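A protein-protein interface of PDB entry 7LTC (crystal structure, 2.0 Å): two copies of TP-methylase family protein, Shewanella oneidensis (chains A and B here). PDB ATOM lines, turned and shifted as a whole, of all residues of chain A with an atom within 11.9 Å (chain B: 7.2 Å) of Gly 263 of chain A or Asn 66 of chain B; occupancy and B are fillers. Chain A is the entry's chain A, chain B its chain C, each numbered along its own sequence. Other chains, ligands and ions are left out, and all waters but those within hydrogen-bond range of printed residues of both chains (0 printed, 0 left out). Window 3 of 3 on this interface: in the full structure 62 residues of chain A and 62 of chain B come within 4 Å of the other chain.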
ATOM      1  N   LEU A 245     -30.053  12.276  18.662  1.00  0.00           N
ATOM      2  CA  LEU A 245     -30.621  10.930  18.742  1.00  0.00           C
ATOM      3  C   LEU A 245     -30.190  10.279  20.059  1.00  0.00           C
ATOM      4  O   LEU A 245     -29.032  10.381  20.471  1.00  0.00           O
ATOM      5  CB  LEU A 245     -30.124  10.089  17.561  1.00  0.00           C
ATOM      6  CG  LEU A 245     -30.624  10.496  16.177  1.00  0.00           C
ATOM      7  CD1 LEU A 245     -29.811   9.791  15.102  1.00  0.00           C
ATOM      8  CD2 LEU A 245     -32.110  10.198  16.018  1.00  0.00           C
ATOM      9  N   TYR A 247     -30.721   6.480  22.392  1.00  0.00           N
ATOM     10  CA  TYR A 247     -30.968   5.060  22.149  1.00  0.00           C
ATOM     11  C   TYR A 247     -32.342   4.652  22.675  1.00  0.00           C
ATOM     12  O   TYR A 247     -32.796   5.091  23.733  1.00  0.00           O
ATOM     13  CB  TYR A 247     -29.899   4.178  22.789  1.00  0.00           C
ATOM     14  CG  TYR A 247     -28.542   4.369  22.175  1.00  0.00           C
ATOM     15  CD1 TYR A 247     -28.289   3.911  20.897  1.00  0.00           C
ATOM     16  CD2 TYR A 247     -27.529   5.028  22.851  1.00  0.00           C
ATOM     17  CE1 TYR A 247     -27.053   4.091  20.303  1.00  0.00           C
ATOM     18  CE2 TYR A 247     -26.286   5.216  22.272  1.00  0.00           C
ATOM     19  CZ  TYR A 247     -26.049   4.744  20.992  1.00  0.00           C
ATOM     20  OH  TYR A 247     -24.833   4.916  20.393  1.00  0.00           O
ATOM     21  N   LEU A 252     -33.934  -2.182  21.596  1.00  0.00           N
ATOM     22  CA  LEU A 252     -32.654  -2.887  21.592  1.00  0.00           C
ATOM     23  C   LEU A 252     -32.784  -4.157  22.449  1.00  0.00           C
ATOM     24  O   LEU A 252     -32.306  -5.225  22.058  1.00  0.00           O
ATOM     25  CB  LEU A 252     -31.540  -1.955  22.088  1.00  0.00           C
ATOM     26  CG  LEU A 252     -31.301  -0.702  21.240  1.00  0.00           C
ATOM     27  CD1 LEU A 252     -30.421   0.300  21.974  1.00  0.00           C
ATOM     28  CD2 LEU A 252     -30.686  -1.047  19.887  1.00  0.00           C
ATOM     29  N   LEU A 255     -34.523  -6.869  20.668  1.00  0.00           N
ATOM     30  CA  LEU A 255     -33.610  -7.419  19.640  1.00  0.00           C
ATOM     31  C   LEU A 255     -32.443  -8.181  20.289  1.00  0.00           C
ATOM     32  O   LEU A 255     -31.626  -8.782  19.567  1.00  0.00           O
ATOM     33  CB  LEU A 255     -33.051  -6.272  18.790  1.00  0.00           C
ATOM     34  CG  LEU A 255     -34.025  -5.564  17.849  1.00  0.00           C
ATOM     35  CD1 LEU A 255     -33.435  -4.257  17.348  1.00  0.00           C
ATOM     36  CD2 LEU A 255     -34.372  -6.443  16.665  1.00  0.00           C
ATOM     37  N   ILE A 257     -29.843  -6.884  21.998  1.00  0.00           N
ATOM     38  CA  ILE A 257     -28.581  -6.160  21.809  1.00  0.00           C
ATOM     39  C   ILE A 257     -28.583  -4.888  22.669  1.00  0.00           C
ATOM     40  O   ILE A 257     -29.617  -4.472  23.189  1.00  0.00           O
ATOM     41  CB  ILE A 257     -28.365  -5.814  20.322  1.00  0.00           C
ATOM     42  CG1 ILE A 257     -29.497  -4.939  19.776  1.00  0.00           C
ATOM     43  CG2 ILE A 257     -28.182  -7.070  19.487  1.00  0.00           C
ATOM     44  CD1 ILE A 257     -29.217  -4.323  18.425  1.00  0.00           C
ATOM     45  N   GLY A 258     -27.403  -4.285  22.793  1.00  0.00           N
ATOM     46  CA  GLY A 258     -27.241  -2.945  23.363  1.00  0.00           C
ATOM     47  C   GLY A 258     -26.484  -2.044  22.397  1.00  0.00           C
ATOM     48  O   GLY A 258     -26.054  -2.504  21.338  1.00  0.00           O
ATOM     49  N   PRO A 259     -26.315  -0.756  22.745  1.00  0.00           N
ATOM     50  CA  PRO A 259     -25.633   0.235  21.903  1.00  0.00           C
ATOM     51  C   PRO A 259     -24.220  -0.207  21.501  1.00  0.00           C
ATOM     52  O   PRO A 259     -23.765   0.082  20.393  1.00  0.00           O
ATOM     53  CB  PRO A 259     -25.537   1.498  22.768  1.00  0.00           C
ATOM     54  CG  PRO A 259     -26.729   1.382  23.661  1.00  0.00           C
ATOM     55  CD  PRO A 259     -26.806  -0.100  23.963  1.00  0.00           C
ATOM     56  N   GLU A 260     -23.548  -0.908  22.399  1.00  0.00           N
ATOM     57  CA  GLU A 260     -22.176  -1.293  22.139  1.00  0.00           C
ATOM     58  C   GLU A 260     -22.134  -2.336  21.007  1.00  0.00           C
ATOM     59  O   GLU A 260     -21.067  -2.560  20.432  1.00  0.00           O
ATOM     60  CB  GLU A 260     -21.503  -1.750  23.439  1.00  0.00           C
ATOM     61  CG  GLU A 260     -21.950  -3.111  23.948  1.00  0.00           C
ATOM     62  CD  GLU A 260     -23.255  -3.157  24.729  1.00  0.00           C
ATOM     63  OE1 GLU A 260     -23.950  -2.120  24.790  1.00  0.00           O
ATOM     64  OE2 GLU A 260     -23.573  -4.236  25.276  1.00  0.00           O
ATOM     65  N   ASP A 261     -23.272  -2.944  20.653  1.00  0.00           N
ATOM     66  CA  ASP A 261     -23.285  -3.974  19.588  1.00  0.00           C
ATOM     67  C   ASP A 261     -23.497  -3.354  18.201  1.00  0.00           C
ATOM     68  O   ASP A 261     -23.299  -4.035  17.190  1.00  0.00           O
ATOM     69  CB  ASP A 261     -24.358  -5.036  19.836  1.00  0.00           C
ATOM     70  CG  ASP A 261     -24.065  -5.869  21.070  1.00  0.00           C
ATOM     71  OD1 ASP A 261     -22.931  -6.380  21.173  1.00  0.00           O
ATOM     72  OD2 ASP A 261     -24.963  -5.984  21.928  1.00  0.00           O
ATOM     73  N   LEU A 262     -23.892  -2.088  18.131  1.00  0.00           N
ATOM     74  CA  LEU A 262     -24.176  -1.464  16.833  1.00  0.00           C
ATOM     75  C   LEU A 262     -22.886  -1.353  16.008  1.00  0.00           C
ATOM     76  O   LEU A 262     -21.833  -0.983  16.531  1.00  0.00           O
ATOM     77  CB  LEU A 262     -24.794  -0.081  17.059  1.00  0.00           C
ATOM     78  CG  LEU A 262     -26.198  -0.065  17.661  1.00  0.00           C
ATOM     79  CD1 LEU A 262     -26.629   1.354  18.001  1.00  0.00           C
ATOM     80  CD2 LEU A 262     -27.198  -0.701  16.714  1.00  0.00           C
ATOM     81  N   GLY A 263     -22.990  -1.660  14.715  1.00  0.00           N
ATOM     82  CA  GLY A 263     -21.867  -1.554  13.784  1.00  0.00           C
ATOM     83  C   GLY A 263     -21.541  -0.110  13.442  1.00  0.00           C
ATOM     84  O   GLY A 263     -22.336   0.810  13.667  1.00  0.00           O
ATOM     85  OXT GLY A 263     -20.455   0.170  12.924  1.00  0.00           O
ATOM     86  N   PHE B  57     -16.777  -1.794  -4.021  1.00  0.00           N
ATOM     87  CA  PHE B  57     -16.375  -1.572  -2.605  1.00  0.00           C
ATOM     88  C   PHE B  57     -17.331  -2.283  -1.635  1.00  0.00           C
ATOM     89  O   PHE B  57     -17.034  -2.386  -0.444  1.00  0.00           O
ATOM     90  CB  PHE B  57     -16.245  -0.074  -2.309  1.00  0.00           C
ATOM     91  CG  PHE B  57     -15.090   0.546  -3.051  1.00  0.00           C
ATOM     92  CD1 PHE B  57     -13.784   0.242  -2.701  1.00  0.00           C
ATOM     93  CD2 PHE B  57     -15.300   1.358  -4.154  1.00  0.00           C
ATOM     94  CE1 PHE B  57     -12.714   0.753  -3.423  1.00  0.00           C
ATOM     95  CE2 PHE B  57     -14.230   1.874  -4.873  1.00  0.00           C
ATOM     96  CZ  PHE B  57     -12.938   1.579  -4.500  1.00  0.00           C
ATOM     97  N   ALA B  59     -19.136  -5.586   0.031  1.00  0.00           N
ATOM     98  CA  ALA B  59     -18.656  -6.938   0.366  1.00  0.00           C
ATOM     99  C   ALA B  59     -18.823  -7.878  -0.839  1.00  0.00           C
ATOM    100  O   ALA B  59     -19.886  -7.908  -1.454  1.00  0.00           O
ATOM    101  CB  ALA B  59     -19.414  -7.445   1.573  1.00  0.00           C
ATOM    102  N   GLU B  63     -17.898 -12.186   2.055  1.00  0.00           N
ATOM    103  CA  GLU B  63     -17.018 -11.447   2.987  1.00  0.00           C
ATOM    104  C   GLU B  63     -17.852 -10.684   4.035  1.00  0.00           C
ATOM    105  O   GLU B  63     -18.933 -10.163   3.731  1.00  0.00           O
ATOM    106  CB  GLU B  63     -16.128 -10.547   2.125  1.00  0.00           C
ATOM    107  CG  GLU B  63     -15.407  -9.431   2.849  1.00  0.00           C
ATOM    108  CD  GLU B  63     -14.881  -8.363   1.905  1.00  0.00           C
ATOM    109  OE1 GLU B  63     -15.435  -8.234   0.793  1.00  0.00           O
ATOM    110  OE2 GLU B  63     -13.913  -7.670   2.279  1.00  0.00           O
ATOM    111  N   VAL B  64     -17.347 -10.660   5.278  1.00  0.00           N
ATOM    112  CA  VAL B  64     -17.890  -9.840   6.380  1.00  0.00           C
ATOM    113  C   VAL B  64     -17.222  -8.462   6.309  1.00  0.00           C
ATOM    114  O   VAL B  64     -16.017  -8.340   6.536  1.00  0.00           O
ATOM    115  CB  VAL B  64     -17.645 -10.472   7.770  1.00  0.00           C
ATOM    116  CG1 VAL B  64     -17.971  -9.500   8.894  1.00  0.00           C
ATOM    117  CG2 VAL B  64     -18.392 -11.781   7.980  1.00  0.00           C
ATOM    118  N   LYS B  65     -18.006  -7.437   5.997  1.00  0.00           N
ATOM    119  CA  LYS B  65     -17.482  -6.082   5.846  1.00  0.00           C
ATOM    120  C   LYS B  65     -18.543  -5.085   6.318  1.00  0.00           C
ATOM    121  O   LYS B  65     -19.688  -5.113   5.868  1.00  0.00           O
ATOM    122  CB  LYS B  65     -17.102  -5.829   4.383  1.00  0.00           C
ATOM    123  CG  LYS B  65     -16.500  -4.467   4.058  1.00  0.00           C
ATOM    124  CD  LYS B  65     -16.126  -4.348   2.591  1.00  0.00           C
ATOM    125  CE  LYS B  65     -15.153  -3.228   2.298  1.00  0.00           C
ATOM    126  NZ  LYS B  65     -14.620  -3.343   0.920  1.00  0.00           N
ATOM    127  N   ASN B  66     -18.133  -4.227   7.237  1.00  0.00           N
ATOM    128  CA  ASN B  66     -18.979  -3.180   7.797  1.00  0.00           C
ATOM    129  C   ASN B  66     -19.227  -2.117   6.711  1.00  0.00           C
ATOM    130  O   ASN B  66     -18.273  -1.638   6.110  1.00  0.00           O
ATOM    131  CB  ASN B  66     -18.312  -2.631   9.063  1.00  0.00           C
ATOM    132  CG  ASN B  66     -19.163  -1.630   9.807  1.00  0.00           C
ATOM    133  OD1 ASN B  66     -19.725  -0.719   9.205  1.00  0.00           O
ATOM    134  ND2 ASN B  66     -19.256  -1.786  11.118  1.00  0.00           N
ATOM    135  N   ARG B  67     -20.486  -1.752   6.446  1.00  0.00           N
ATOM    136  CA  ARG B  67     -20.808  -0.809   5.342  1.00  0.00           C
ATOM    137  C   ARG B  67     -20.137   0.558   5.579  1.00  0.00           C
ATOM    138  O   ARG B  67     -19.901   1.290   4.621  1.00  0.00           O
ATOM    139  CB  ARG B  67     -22.326  -0.694   5.140  1.00  0.00           C
ATOM    140  CG  ARG B  67     -22.896  -1.727   4.176  1.00  0.00           C
ATOM    141  CD  ARG B  67     -24.304  -1.459   3.659  1.00  0.00           C
ATOM    142  NE  ARG B  67     -25.113  -0.552   4.465  1.00  0.00           N
ATOM    143  CZ  ARG B  67     -25.917  -0.922   5.456  1.00  0.00           C
ATOM    144  NH1 ARG B  67     -25.912  -2.171   5.893  1.00  0.00           N
ATOM    145  NH2 ARG B  67     -26.721  -0.032   6.012  1.00  0.00           N
ATOM    146  N   ARG B  68     -19.824   0.916   6.830  1.00  0.00           N
ATOM    147  CA  ARG B  68     -19.066   2.161   7.128  1.00  0.00           C
ATOM    148  C   ARG B  68     -17.714   2.147   6.401  1.00  0.00           C
ATOM    149  O   ARG B  68     -17.243   3.193   5.942  1.00  0.00           O
ATOM    150  CB  ARG B  68     -18.773   2.319   8.626  1.00  0.00           C
ATOM    151  CG  ARG B  68     -19.978   2.574   9.521  1.00  0.00           C
ATOM    152  CD  ARG B  68     -19.506   2.752  10.957  1.00  0.00           C
ATOM    153  NE  ARG B  68     -20.578   2.854  11.939  1.00  0.00           N
ATOM    154  CZ  ARG B  68     -21.235   3.973  12.239  1.00  0.00           C
ATOM    155  NH1 ARG B  68     -20.922   5.115  11.650  1.00  0.00           N
ATOM    156  NH2 ARG B  68     -22.208   3.942  13.132  1.00  0.00           N
ATOM    157  N   ASP B  69     -17.085   0.971   6.344  1.00  0.00           N
ATOM    158  CA  ASP B  69     -15.793   0.785   5.654  1.00  0.00           C
ATOM    159  C   ASP B  69     -15.991   0.867   4.134  1.00  0.00           C
ATOM    160  O   ASP B  69     -15.164   1.451   3.434  1.00  0.00           O
ATOM    161  CB  ASP B  69     -15.124  -0.530   6.062  1.00  0.00           C
ATOM    162  CG  ASP B  69     -14.738  -0.553   7.529  1.00  0.00           C
ATOM    163  OD1 ASP B  69     -14.370   0.520   8.049  1.00  0.00           O
ATOM    164  OD2 ASP B  69     -14.828  -1.633   8.148  1.00  0.00           O
ATOM    165  N   THR B  70     -17.058   0.266   3.622  1.00  0.00           N
ATOM    166  CA  THR B  70     -17.391   0.395   2.202  1.00  0.00           C
ATOM    167  C   THR B  70     -17.510   1.880   1.820  1.00  0.00           C
ATOM    168  O   THR B  70     -16.936   2.318   0.816  1.00  0.00           O
ATOM    169  CB  THR B  70     -18.684  -0.368   1.880  1.00  0.00           C
ATOM    170  OG1 THR B  70     -18.389  -1.764   1.936  1.00  0.00           O
ATOM    171  CG2 THR B  70     -19.260  -0.032   0.521  1.00  0.00           C
ATOM    172  N   TYR B  71     -18.267   2.644   2.614  1.00  0.00           N
ATOM    173  CA  TYR B  71     -18.532   4.075   2.324  1.00  0.00           C
ATOM    174  C   TYR B  71     -17.221   4.869   2.411  1.00  0.00           C
ATOM    175  O   TYR B  71     -16.929   5.670   1.522  1.00  0.00           O
ATOM    176  CB  TYR B  71     -19.643   4.632   3.225  1.00  0.00           C
ATOM    177  CG  TYR B  71     -20.949   3.879   3.116  1.00  0.00           C
ATOM    178  CD1 TYR B  71     -21.344   3.325   1.909  1.00  0.00           C
ATOM    179  CD2 TYR B  71     -21.792   3.710   4.205  1.00  0.00           C
ATOM    180  CE1 TYR B  71     -22.533   2.622   1.782  1.00  0.00           C
ATOM    181  CE2 TYR B  71     -22.987   3.013   4.095  1.00  0.00           C
ATOM    182  CZ  TYR B  71     -23.358   2.465   2.879  1.00  0.00           C
ATOM    183  OH  TYR B  71     -24.529   1.774   2.746  1.00  0.00           O
ATOM    184  N   GLU B  72     -16.434   4.635   3.459  1.00  0.00           N
ATOM    185  CA  GLU B  72     -15.108   5.262   3.593  1.00  0.00           C
ATOM    186  C   GLU B  72     -14.269   4.989   2.334  1.00  0.00           C
ATOM    187  O   GLU B  72     -13.640   5.904   1.810  1.00  0.00           O
ATOM    188  CB  GLU B  72     -14.414   4.765   4.866  1.00  0.00           C
ATOM    189  CG  GLU B  72     -13.046   5.380   5.100  1.00  0.00           C
ATOM    190  CD  GLU B  72     -13.041   6.898   5.127  1.00  0.00           C
ATOM    191  OE1 GLU B  72     -14.051   7.483   5.569  1.00  0.00           O
ATOM    192  OE2 GLU B  72     -12.030   7.493   4.700  1.00  0.00           O
ATOM    193  N   GLN B  73     -14.262   3.747   1.852  1.00  0.00           N
ATOM    194  CA  GLN B  73     -13.457   3.366   0.677  1.00  0.00           C
ATOM    195  C   GLN B  73     -13.974   4.067  -0.590  1.00  0.00           C
ATOM    196  O   GLN B  73     -13.174   4.478  -1.428  1.00  0.00           O
ATOM    197  CB  GLN B  73     -13.429   1.842   0.538  1.00  0.00           C
ATOM    198  CG  GLN B  73     -12.498   1.175   1.545  1.00  0.00           C
ATOM    199  CD  GLN B  73     -12.651  -0.326   1.585  1.00  0.00           C
ATOM    200  OE1 GLN B  73     -13.218  -0.932   0.679  1.00  0.00           O
ATOM    201  NE2 GLN B  73     -12.150  -0.943   2.644  1.00  0.00           N
ATOM    202  N   PHE B 152     -33.629   1.708  16.479  1.00  0.00           N
ATOM    203  CA  PHE B 152     -32.488   1.782  17.399  1.00  0.00           C
ATOM    204  C   PHE B 152     -32.495   3.083  18.209  1.00  0.00           C
ATOM    205  O   PHE B 152     -31.852   3.173  19.257  1.00  0.00           O
ATOM    206  CB  PHE B 152     -31.176   1.700  16.624  1.00  0.00           C
ATOM    207  CG  PHE B 152     -30.989   0.427  15.846  1.00  0.00           C
ATOM    208  CD1 PHE B 152     -31.563  -0.765  16.258  1.00  0.00           C
ATOM    209  CD2 PHE B 152     -30.212   0.426  14.702  1.00  0.00           C
ATOM    210  CE1 PHE B 152     -31.370  -1.928  15.530  1.00  0.00           C
ATOM    211  CE2 PHE B 152     -30.019  -0.737  13.977  1.00  0.00           C
ATOM    212  CZ  PHE B 152     -30.596  -1.913  14.393  1.00  0.00           C
ATOM    213  N   GLU B 173     -31.020  -4.679  11.225  1.00  0.00           N
ATOM    214  CA  GLU B 173     -29.755  -5.372  10.961  1.00  0.00           C
ATOM    215  C   GLU B 173     -28.603  -4.523  11.519  1.00  0.00           C
ATOM    216  O   GLU B 173     -28.020  -3.695  10.814  1.00  0.00           O
ATOM    217  CB  GLU B 173     -29.611  -5.667   9.466  1.00  0.00           C
ATOM    218  CG  GLU B 173     -28.641  -6.794   9.167  1.00  0.00           C
ATOM    219  CD  GLU B 173     -27.213  -6.512   9.603  1.00  0.00           C
ATOM    220  OE1 GLU B 173     -26.466  -5.898   8.811  1.00  0.00           O
ATOM    221  OE2 GLU B 173     -26.852  -6.894  10.737  1.00  0.00           O
ATOM    222  N   HIS B 174     -28.273  -4.760  12.789  1.00  0.00           N
ATOM    223  CA  HIS B 174     -27.449  -3.838  13.591  1.00  0.00           C
ATOM    224  C   HIS B 174     -25.953  -3.928  13.252  1.00  0.00           C
ATOM    225  O   HIS B 174     -25.206  -3.025  13.633  1.00  0.00           O
ATOM    226  CB  HIS B 174     -27.657  -4.101  15.091  1.00  0.00           C
ATOM    227  CG  HIS B 174     -27.102  -5.410  15.534  1.00  0.00           C
ATOM    228  ND1 HIS B 174     -27.822  -6.584  15.432  1.00  0.00           N
ATOM    229  CD2 HIS B 174     -25.897  -5.746  16.047  1.00  0.00           C
ATOM    230  CE1 HIS B 174     -27.093  -7.586  15.878  1.00  0.00           C
ATOM    231  NE2 HIS B 174     -25.906  -7.097  16.260  1.00  0.00           N
ATOM    232  N   THR B 175     -25.499  -4.976  12.556  1.00  0.00           N
ATOM    233  CA  THR B 175     -24.048  -5.180  12.344  1.00  0.00           C
ATOM    234  C   THR B 175     -23.534  -4.366  11.141  1.00  0.00           C
ATOM    235  O   THR B 175     -22.328  -4.152  11.018  1.00  0.00           O
ATOM    236  CB  THR B 175     -23.701  -6.665  12.158  1.00  0.00           C
ATOM    237  OG1 THR B 175     -24.287  -7.110  10.933  1.00  0.00           O
ATOM    238  CG2 THR B 175     -24.152  -7.522  13.323  1.00  0.00           C
ATOM    239  N   LEU B 176     -24.433  -3.919  10.263  1.00  0.00           N
ATOM    240  CA  LEU B 176     -24.080  -3.280   8.968  1.00  0.00           C
ATOM    241  C   LEU B 176     -23.206  -4.221   8.125  1.00  0.00           C
ATOM    242  O   LEU B 176     -22.369  -3.761   7.343  1.00  0.00           O
ATOM    243  CB  LEU B 176     -23.362  -1.945   9.199  1.00  0.00           C
ATOM    244  CG  LEU B 176     -24.051  -0.935  10.117  1.00  0.00           C
ATOM    245  CD1 LEU B 176     -23.317   0.400  10.094  1.00  0.00           C
ATOM    246  CD2 LEU B 176     -25.507  -0.740   9.730  1.00  0.00           C
ATOM    247  N   THR B 177     -23.406  -5.531   8.258  1.00  0.00           N
ATOM    248  CA  THR B 177     -22.620  -6.489   7.475  1.00  0.00           C
ATOM    249  C   THR B 177     -23.529  -7.452   6.697  1.00  0.00           C
ATOM    250  O   THR B 177     -23.022  -8.270   5.929  1.00  0.00           O
ATOM    251  CB  THR B 177     -21.653  -7.307   8.342  1.00  0.00           C
ATOM    252  OG1 THR B 177     -22.430  -8.216   9.124  1.00  0.00           O
ATOM    253  CG2 THR B 177     -20.770  -6.460   9.232  1.00  0.00           C
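OG1 of Thr 177 of chain B lies within hydrogen-bond range of OG1 of Thr 175 of chain B (2.8 Å). The side-chain amide oxygen (OD1) of Asn 66 of chain B sits at hydrogen-bond distance from the backbone NH (N) of Arg 68 of chain B (2.9 Å). OE2 of Glu 173 of chain B is in hydrogen-bond range of OG1 of Thr 175 of chain B (2.6 Å). N of Ile 257 of chain A sits at hydrogen-bond distance from O of Leu 252 of chain A (3.0 Å). The backbone NH (N) of Leu 176 of chain B sits at hydrogen-bond distance from the side-chain carboxylate (OE1) of Glu 173 of chain B, at 3.2 Å. The backbone carbonyl oxygen (O) of Leu 176 of chain B sits at hydrogen-bond distance from the backbone NH (N) of Arg 67 of chain B, at 2.9 Å.
Of the 11 printed residues of chain A, 7 touch a printed residue of chain B. Hydrophobic or aromatic side chains of chain A within 4 Å of the printed part of chain B: Tyr 247, Leu 252, Leu 255, Ile 257 and Leu 262. Along chain A the printed residues that touch a printed residue of chain B span positions 247 to 263. Of the 19 printed residues of chain B, 6 touch a printed residue of chain A. Printed residues of chain B that touch a printed residue of chain A: Asn 66, Arg 68, Phe 152, His 174, Thr 175 and Leu 176. Hydrophobic or aromatic side chains of chain B that line the printed part of chain A: Phe 152, His 174 and Leu 176. Among the printed residues, no Asp or Glu carboxylate lies within 4 Å of a Lys or Arg side-chain nitrogen of the other chain.
Of chain B, only Asn 66, Arg 68, His 174, Thr 175 and Leu 176 come within 4 Å of Gly 263 of chain A. Of chain A, only Gly 263 (2.9 Å) comes within 4 Å of Asn 66 of chain B. No residue of chain A comes within 4 Å of Val 64 of chain B. No residue of chain A comes within 4 Å of Lys 65 of chain B. No residue of chain A comes within 4 Å of Arg 67 of chain B. Of chain A, only Gly 263 comes within 4 Å of Arg 68 of chain B. Leu 176 of chain B touches just one residue of chain A: Gly 263. Thr 177 of chain B touches none of the printed residues of chain A. Of the printed residues of chain B, Leu 255 of chain A touches Phe 152 (3.6 Å). Printed residues of chain B within 4 Å of Ile 257 of chain A: His 174 (3.7 Å). Of the printed residues of chain B, Asp 261 of chain A touches His 174. Glu 63 of chain B touches none of the printed residues of chain A. The nearest residue of chain B that does not touch Gly 263 of chain A is Glu 173 of chain B (6.7 Å). The nearest printed residue of chain B that does not touch Ile 257 of chain A is Phe 152 of chain B (4.3 Å).
No position is printed for both chains.
The chain-end carboxylate of Gly 263 of chain A is in salt-bridge range of the guanidinium group of Arg 68 of chain B (2.9 Å). O of His 174 of chain B is in hydrogen-bond range of N of Gly 263 of chain A, at 2.8 Å. OXT of Gly 263 of chain A is in hydrogen-bond range of ND2 of Asn 66 of chain B (2.9 Å).
Among the printed residues, pairs that only touch across the chains: Asp 261 of chain A with His 174 of chain B, Tyr 247 of chain A with Phe 152 of chain B, Leu 255 of chain A with Phe 152 of chain B, Ile 257 of chain A with His 174 of chain B, Leu 262 of chain A with His 174 of chain B, Gly 263 of chain A with Leu 176 of chain B, Leu 252 of chain A with Phe 152 of chain B, Leu 262 of chain A with Phe 152 of chain B and Gly 263 of chain A with Thr 175 of chain B.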
